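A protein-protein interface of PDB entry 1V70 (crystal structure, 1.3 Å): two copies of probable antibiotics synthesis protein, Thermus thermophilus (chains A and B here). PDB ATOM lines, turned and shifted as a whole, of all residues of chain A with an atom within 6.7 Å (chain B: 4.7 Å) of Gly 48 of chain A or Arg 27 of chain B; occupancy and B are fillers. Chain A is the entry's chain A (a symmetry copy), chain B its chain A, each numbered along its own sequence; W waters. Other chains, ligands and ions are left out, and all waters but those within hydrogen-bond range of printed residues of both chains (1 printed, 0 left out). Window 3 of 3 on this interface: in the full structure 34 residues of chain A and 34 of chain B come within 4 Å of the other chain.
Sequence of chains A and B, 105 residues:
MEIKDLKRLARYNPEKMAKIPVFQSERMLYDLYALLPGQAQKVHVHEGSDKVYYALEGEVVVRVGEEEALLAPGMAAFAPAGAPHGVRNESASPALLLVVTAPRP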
ATOM      1  N   ARG A  27      20.540  27.016 -23.695  1.00  0.00           N
ATOM      2  CA  ARG A  27      20.478  27.428 -22.303  1.00  0.00           C
ATOM      3  C   ARG A  27      20.070  26.343 -21.315  1.00  0.00           C
ATOM      4  O   ARG A  27      20.407  26.432 -20.139  1.00  0.00           O
ATOM      5  CB  ARG A  27      19.556  28.641 -22.161  1.00  0.00           C
ATOM      6  CG  ARG A  27      20.223  29.945 -22.584  1.00  0.00           C
ATOM      7  CD  ARG A  27      19.229  31.086 -22.659  1.00  0.00           C
ATOM      8  NE  ARG A  27      18.413  31.010 -23.865  1.00  0.00           N
ATOM      9  CZ  ARG A  27      18.888  31.163 -25.097  1.00  0.00           C
ATOM     10  NH1 ARG A  27      20.179  31.404 -25.288  1.00  0.00           N
ATOM     11  NH2 ARG A  27      18.074  31.073 -26.140  1.00  0.00           N
ATOM     12  N   VAL A  45      30.295  13.650 -14.500  1.00  0.00           N
ATOM     13  CA  VAL A  45      30.592  15.021 -14.135  1.00  0.00           C
ATOM     14  C   VAL A  45      30.385  15.951 -15.319  1.00  0.00           C
ATOM     15  O   VAL A  45      30.826  15.660 -16.432  1.00  0.00           O
ATOM     16  CB  VAL A  45      32.063  15.168 -13.662  1.00  0.00           C
ATOM     17  CG1 VAL A  45      32.399  16.636 -13.448  1.00  0.00           C
ATOM     18  CG2 VAL A  45      32.282  14.388 -12.381  1.00  0.00           C
ATOM     19  N   HIS A  46      29.688  17.056 -15.075  1.00  0.00           N
ATOM     20  CA  HIS A  46      29.466  18.069 -16.100  1.00  0.00           C
ATOM     21  C   HIS A  46      30.397  19.208 -15.718  1.00  0.00           C
ATOM     22  O   HIS A  46      30.251  19.798 -14.648  1.00  0.00           O
ATOM     23  CB  HIS A  46      28.024  18.577 -16.087  1.00  0.00           C
ATOM     24  CG  HIS A  46      27.034  17.616 -16.664  1.00  0.00           C
ATOM     25  ND1 HIS A  46      27.157  17.092 -17.933  1.00  0.00           N
ATOM     26  CD2 HIS A  46      25.885  17.107 -16.158  1.00  0.00           C
ATOM     27  CE1 HIS A  46      26.130  16.301 -18.182  1.00  0.00           C
ATOM     28  NE2 HIS A  46      25.343  16.294 -17.122  1.00  0.00           N
ATOM     29  N   GLU A  47      31.356  19.512 -16.587  1.00  0.00           N
ATOM     30  CA  GLU A  47      32.320  20.571 -16.322  1.00  0.00           C
ATOM     31  C   GLU A  47      31.703  21.934 -16.029  1.00  0.00           C
ATOM     32  O   GLU A  47      32.155  22.640 -15.126  1.00  0.00           O
ATOM     33  CB  GLU A  47      33.294  20.697 -17.498  1.00  0.00           C
ATOM     34  CG  GLU A  47      32.631  21.018 -18.830  1.00  0.00           C
ATOM     35  N   GLY A  48      30.674  22.311 -16.782  1.00  0.00           N
ATOM     36  CA  GLY A  48      30.071  23.613 -16.563  1.00  0.00           C
ATOM     37  C   GLY A  48      28.559  23.679 -16.572  1.00  0.00           C
ATOM     38  O   GLY A  48      27.986  24.695 -16.959  1.00  0.00           O
ATOM     39  N   SER A  49      27.904  22.605 -16.146  1.00  0.00           N
ATOM     40  CA  SER A  49      26.445  22.584 -16.107  1.00  0.00           C
ATOM     41  C   SER A  49      25.941  22.103 -14.758  1.00  0.00           C
ATOM     42  O   SER A  49      26.514  21.190 -14.165  1.00  0.00           O
ATOM     43  CB  SER A  49      25.885  21.661 -17.194  1.00  0.00           C
ATOM     44  OG  SER A  49      26.186  22.128 -18.498  1.00  0.00           O
ATOM     45  N   ASP A  50      24.876  22.730 -14.266  1.00  0.00           N
ATOM     46  CA  ASP A  50      24.267  22.316 -13.010  1.00  0.00           C
ATOM     47  C   ASP A  50      23.087  21.440 -13.404  1.00  0.00           C
ATOM     48  O   ASP A  50      22.526  21.596 -14.487  1.00  0.00           O
ATOM     49  CB  ASP A  50      23.748  23.514 -12.204  1.00  0.00           C
ATOM     50  CG  ASP A  50      24.860  24.387 -11.658  1.00  0.00           C
ATOM     51  OD1 ASP A  50      25.938  23.857 -11.328  1.00  0.00           O
ATOM     52  OD2 ASP A  50      24.645  25.610 -11.541  1.00  0.00           O
ATOM     53  N   PHE A  78      19.953  18.881  -5.966  1.00  0.00           N
ATOM     54  CA  PHE A  78      20.809  19.705  -6.813  1.00  0.00           C
ATOM     55  C   PHE A  78      22.220  19.121  -6.966  1.00  0.00           C
ATOM     56  O   PHE A  78      22.875  18.802  -5.976  1.00  0.00           O
ATOM     57  CB  PHE A  78      20.905  21.105  -6.193  1.00  0.00           C
ATOM     58  CG  PHE A  78      21.641  22.107  -7.037  1.00  0.00           C
ATOM     59  CD1 PHE A  78      21.014  22.728  -8.110  1.00  0.00           C
ATOM     60  CD2 PHE A  78      22.963  22.437  -6.752  1.00  0.00           C
ATOM     61  CE1 PHE A  78      21.692  23.669  -8.890  1.00  0.00           C
ATOM     62  CE2 PHE A  78      23.649  23.375  -7.526  1.00  0.00           C
ATOM     63  CZ  PHE A  78      23.011  23.991  -8.595  1.00  0.00           C
ATOM     64  N   PRO A  80      25.617  20.330  -8.440  1.00  0.00           N
ATOM     65  CA  PRO A  80      26.383  21.429  -9.032  1.00  0.00           C
ATOM     66  C   PRO A  80      27.471  20.971  -9.994  1.00  0.00           C
ATOM     67  O   PRO A  80      28.001  19.867  -9.875  1.00  0.00           O
ATOM     68  CB  PRO A  80      26.953  22.143  -7.810  1.00  0.00           C
ATOM     69  CG  PRO A  80      27.185  21.018  -6.854  1.00  0.00           C
ATOM     70  CD  PRO A  80      25.923  20.184  -7.006  1.00  0.00           C
ATOM     71  N   ALA A  81      27.792  21.834 -10.953  1.00  0.00           N
ATOM     72  CA  ALA A  81      28.824  21.544 -11.939  1.00  0.00           C
ATOM     73  C   ALA A  81      30.099  21.100 -11.236  1.00  0.00           C
ATOM     74  O   ALA A  81      30.505  21.690 -10.231  1.00  0.00           O
ATOM     75  CB  ALA A  81      29.097  22.786 -12.781  1.00  0.00           C
ATOM     76  N   GLY A  82      30.726  20.054 -11.762  1.00  0.00           N
ATOM     77  CA  GLY A  82      31.954  19.551 -11.178  1.00  0.00           C
ATOM     78  C   GLY A  82      31.765  18.403 -10.203  1.00  0.00           C
ATOM     79  O   GLY A  82      32.706  17.661  -9.920  1.00  0.00           O
ATOM     80  N   ALA A 102      21.560  22.835 -16.970  1.00  0.00           N
ATOM     81  CA  ALA A 102      21.838  24.159 -17.523  1.00  0.00           C
ATOM     82  C   ALA A 102      23.259  24.633 -17.243  1.00  0.00           C
ATOM     83  O   ALA A 102      23.745  24.545 -16.118  1.00  0.00           O
ATOM     84  CB  ALA A 102      20.839  25.172 -16.968  1.00  0.00           C
ATOM     85  N   PRO A 103      23.956  25.110 -18.286  1.00  0.00           N
ATOM     86  CA  PRO A 103      23.435  25.186 -19.654  1.00  0.00           C
ATOM     87  C   PRO A 103      23.494  23.803 -20.300  1.00  0.00           C
ATOM     88  O   PRO A 103      23.881  22.828 -19.649  1.00  0.00           O
ATOM     89  CB  PRO A 103      24.376  26.185 -20.325  1.00  0.00           C
ATOM     90  CG  PRO A 103      25.669  25.934 -19.624  1.00  0.00           C
ATOM     91  CD  PRO A 103      25.249  25.809 -18.176  1.00  0.00           C
ATOM     92  N   ARG A 104      23.100  23.706 -21.564  1.00  0.00           N
ATOM     93  CA  ARG A 104      23.144  22.422 -22.255  1.00  0.00           C
ATOM     94  C   ARG A 104      24.603  21.986 -22.352  1.00  0.00           C
ATOM     95  O   ARG A 104      25.457  22.755 -22.787  1.00  0.00           O
ATOM     96  CB  ARG A 104      22.533  22.551 -23.655  1.00  0.00           C
ATOM     97  CG  ARG A 104      22.533  21.258 -24.461  1.00  0.00           C
ATOM     98  CD  ARG A 104      21.642  21.372 -25.692  1.00  0.00           C
ATOM     99  NE  ARG A 104      22.034  22.480 -26.557  1.00  0.00           N
ATOM    100  CZ  ARG A 104      21.358  22.862 -27.637  1.00  0.00           C
ATOM    101  NH1 ARG A 104      20.249  22.225 -27.991  1.00  0.00           N
ATOM    102  NH2 ARG A 104      21.790  23.884 -28.364  1.00  0.00           N
ATOM    103  N   SER B  25      21.874  29.332  -8.727  1.00  0.00           N
ATOM    104  CA  SER B  25      23.271  29.423  -9.125  1.00  0.00           C
ATOM    105  C   SER B  25      23.270  30.382 -10.301  1.00  0.00           C
ATOM    106  O   SER B  25      22.205  30.768 -10.783  1.00  0.00           O
ATOM    107  CB  SER B  25      23.807  28.060  -9.566  1.00  0.00           C
ATOM    108  OG  SER B  25      23.261  27.678 -10.817  1.00  0.00           O
ATOM    109  N   GLU B  26      24.450  30.775 -10.763  1.00  0.00           N
ATOM    110  CA  GLU B  26      24.516  31.689 -11.893  1.00  0.00           C
ATOM    111  C   GLU B  26      23.949  30.999 -13.128  1.00  0.00           C
ATOM    112  O   GLU B  26      23.529  31.655 -14.084  1.00  0.00           O
ATOM    113  CB  GLU B  26      25.963  32.124 -12.153  1.00  0.00           C
ATOM    114  CG  GLU B  26      26.887  31.038 -12.694  1.00  0.00           C
ATOM    115  N   ARG B  27      23.917  29.670 -13.089  1.00  0.00           N
ATOM    116  CA  ARG B  27      23.422  28.892 -14.211  1.00  0.00           C
ATOM    117  C   ARG B  27      21.910  28.719 -14.273  1.00  0.00           C
ATOM    118  O   ARG B  27      21.365  28.494 -15.349  1.00  0.00           O
ATOM    119  CB  ARG B  27      24.109  27.525 -14.240  1.00  0.00           C
ATOM    120  CG  ARG B  27      25.517  27.583 -14.819  1.00  0.00           C
ATOM    121  CD  ARG B  27      26.260  26.276 -14.623  1.00  0.00           C
ATOM    122  NE  ARG B  27      26.734  26.128 -13.252  1.00  0.00           N
ATOM    123  CZ  ARG B  27      27.666  26.898 -12.698  1.00  0.00           C
ATOM    124  NH1 ARG B  27      28.229  27.871 -13.401  1.00  0.00           N
ATOM    125  NH2 ARG B  27      28.035  26.696 -11.441  1.00  0.00           N
ATOM    126  N   MET B  28      21.224  28.820 -13.140  1.00  0.00           N
ATOM    127  CA  MET B  28      19.771  28.674 -13.171  1.00  0.00           C
ATOM    128  C   MET B  28      19.061  29.034 -11.882  1.00  0.00           C
ATOM    129  O   MET B  28      19.647  29.025 -10.798  1.00  0.00           O
ATOM    130  CB  MET B  28      19.375  27.233 -13.528  1.00  0.00           C
ATOM    131  CG  MET B  28      19.457  26.252 -12.352  1.00  0.00           C
ATOM    132  SD  MET B  28      18.583  24.659 -12.582  1.00  0.00           S
ATOM    133  CE  MET B  28      19.906  23.653 -13.235  1.00  0.00           C
ATOM    134  N   THR B 101      14.454  29.030 -14.670  1.00  0.00           N
ATOM    135  CA  THR B 101      14.947  30.103 -15.526  1.00  0.00           C
ATOM    136  C   THR B 101      16.447  29.894 -15.692  1.00  0.00           C
ATOM    137  O   THR B 101      17.160  29.694 -14.709  1.00  0.00           O
ATOM    138  CB  THR B 101      14.707  31.485 -14.889  1.00  0.00           C
ATOM    139  OG1 THR B 101      13.326  31.615 -14.530  1.00  0.00           O
ATOM    140  CG2 THR B 101      15.076  32.592 -15.868  1.00  0.00           C
ATOM    141  N   ALA B 102      16.924  29.935 -16.932  1.00  0.00           N
ATOM    142  CA  ALA B 102      18.345  29.725 -17.199  1.00  0.00           C
ATOM    143  C   ALA B 102      18.845  30.510 -18.405  1.00  0.00           C
ATOM    144  O   ALA B 102      18.221  30.508 -19.464  1.00  0.00           O
ATOM    145  CB  ALA B 102      18.619  28.236 -17.404  1.00  0.00           C
ATOM    146  N   PRO B 103      19.968  31.227 -18.241  1.00  0.00           N
ATOM    147  CA  PRO B 103      20.717  31.300 -16.982  1.00  0.00           C
ATOM    148  C   PRO B 103      20.012  32.260 -16.025  1.00  0.00           C
ATOM    149  O   PRO B 103      18.945  32.788 -16.347  1.00  0.00           O
ATOM    150  CB  PRO B 103      22.084  31.815 -17.425  1.00  0.00           C
ATOM    151  CG  PRO B 103      21.742  32.688 -18.585  1.00  0.00           C
ATOM    152  CD  PRO B 103      20.718  31.866 -19.336  1.00  0.00           C
ATOM    153  N   ARG B 104      20.589  32.477 -14.849  1.00  0.00           N
ATOM    154  CA  ARG B 104      19.987  33.394 -13.888  1.00  0.00           C
ATOM    155  C   ARG B 104      19.995  34.793 -14.500  1.00  0.00           C
ATOM    156  O   ARG B 104      21.028  35.261 -14.975  1.00  0.00           O
ATOM    157  CB  ARG B 104      20.776  33.382 -12.575  1.00  0.00           C
ATOM    158  CG  ARG B 104      20.225  34.314 -11.503  1.00  0.00           C
ATOM    159  CD  ARG B 104      20.848  34.024 -10.143  1.00  0.00           C
ATOM    160  NE  ARG B 104      22.304  34.127 -10.169  1.00  0.00           N
ATOM    161  CZ  ARG B 104      23.095  33.821  -9.144  1.00  0.00           C
ATOM    162  NH1 ARG B 104      22.573  33.389  -8.004  1.00  0.00           N
ATOM    163  NH2 ARG B 104      24.410  33.944  -9.260  1.00  0.00           N
HETATM  164  O   HOH W   1      26.888  25.403  -9.156  1.00  0.00           O
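Of the printed residues of chain B, Arg 27 of chain A touches Ala 102 (3.4 Å) and Pro 103 (3.7 Å). Of chain B, only Arg 27 comes within 4 Å of Gly 48 of chain A. Of the printed residues of chain B, Ser 49 of chain A touches Arg 27. Of the printed residues of chain B, Ala 102 of chain A touches Arg 27 (3.4 Å) and Ala 102 (3.8 Å). Of the printed residues of chain A, Arg 27 of chain B touches Gly 48 (3.3 Å), Ser 49 (3.98 Å), Asp 50 (2.7 Å), Ala 102 (3.4 Å) and Pro 103 (3.7 Å). Of the printed residues of chain A, Ala 102 of chain B touches Arg 27 and Ala 102. The nearest printed residue of chain B that does not touch Ser 49 of chain A is Met 28 of chain B (6.4 Å).
The side-chain hydroxyl (OG) of Ser 25 of chain B is in hydrogen-bond range of the side-chain carboxylate (OD2) of Asp 50 of chain A (2.6 Å). NE of Arg 27 of chain B lies within salt-bridge range of OD2 of Asp 50 of chain A.
Printed residues of chain B that touch a printed residue of chain A: Ser 25, Arg 27, Met 28, Ala 102 and Pro 103. Hydrophobic or aromatic side chains of chain B within 4 Å of the printed part of chain A: Met 28, Ala 102 and Pro 103. Printed residues of chain A that touch a printed residue of chain B: Arg 27, Gly 48, Ser 49, Asp 50, Ala 102 and Pro 103. Hydrophobic or aromatic side chains of chain A that line the printed part of chain B: Ala 102 and Pro 103.
Arg 27 of chain A touches Ala 102 of chain B, and with the chains exchanged Ala 102 of chain A touches Arg 27 of chain B. Arg 27 of chain A touches Pro 103 of chain B, and with the chains exchanged Pro 103 of chain A touches Arg 27 of chain B. Ala 102 of chain B touches its own counterpart, Ala 102 of chain A. 4 positions are printed for both chains.
Water W1 lies within hydrogen-bond range of the side-chain carboxylate (OD1) of Asp 50 of chain A and the guanidinium group (NH2) of Arg 27 of chain B.
Among the printed residues, pairs that only touch across the chains: Arg 27 of chain A with Ala 102 of chain B (3.4 Å), Arg 27 of chain A with Pro 103 of chain B (3.7 Å), Gly 48 of chain A with Arg 27 of chain B (3.3 Å), Ser 49 of chain A with Arg 27 of chain B (3.98 Å), Asp 50 of chain A with Met 28 of chain B (3.6 Å), Ala 102 of chain A with Arg 27 of chain B (3.4 Å), Ala 102 of chain A with Ala 102 of chain B (3.8 Å) and Pro 103 of chain A with Arg 27 of chain B (3.7 Å).
The side-chain hydroxyl of Ser 25 of chain B lies close to the backbone NH of Arg 27 of chain B, at 3.1 Å. N of Met 28 of chain B sits at hydrogen-bond distance from OG of Ser 25 of chain B (3.3 Å). O of Ser 25 of chain B is in hydrogen-bond range of NE of Arg 104 of chain B, at 3.4 Å. The side-chain hydroxyl (OG) of Ser 49 of chain A lies within hydrogen-bond range of the backbone carbonyl oxygen (O) of Pro 103 of chain A (2.7 Å). The backbone NH (N) of Ala 81 of chain A is in hydrogen-bond range of the side-chain carboxylate (OD1) of Asp 50 of chain A, at 2.8 Å. N of Asp 50 of chain A lies within hydrogen-bond range of O of Ala 102 of chain A.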
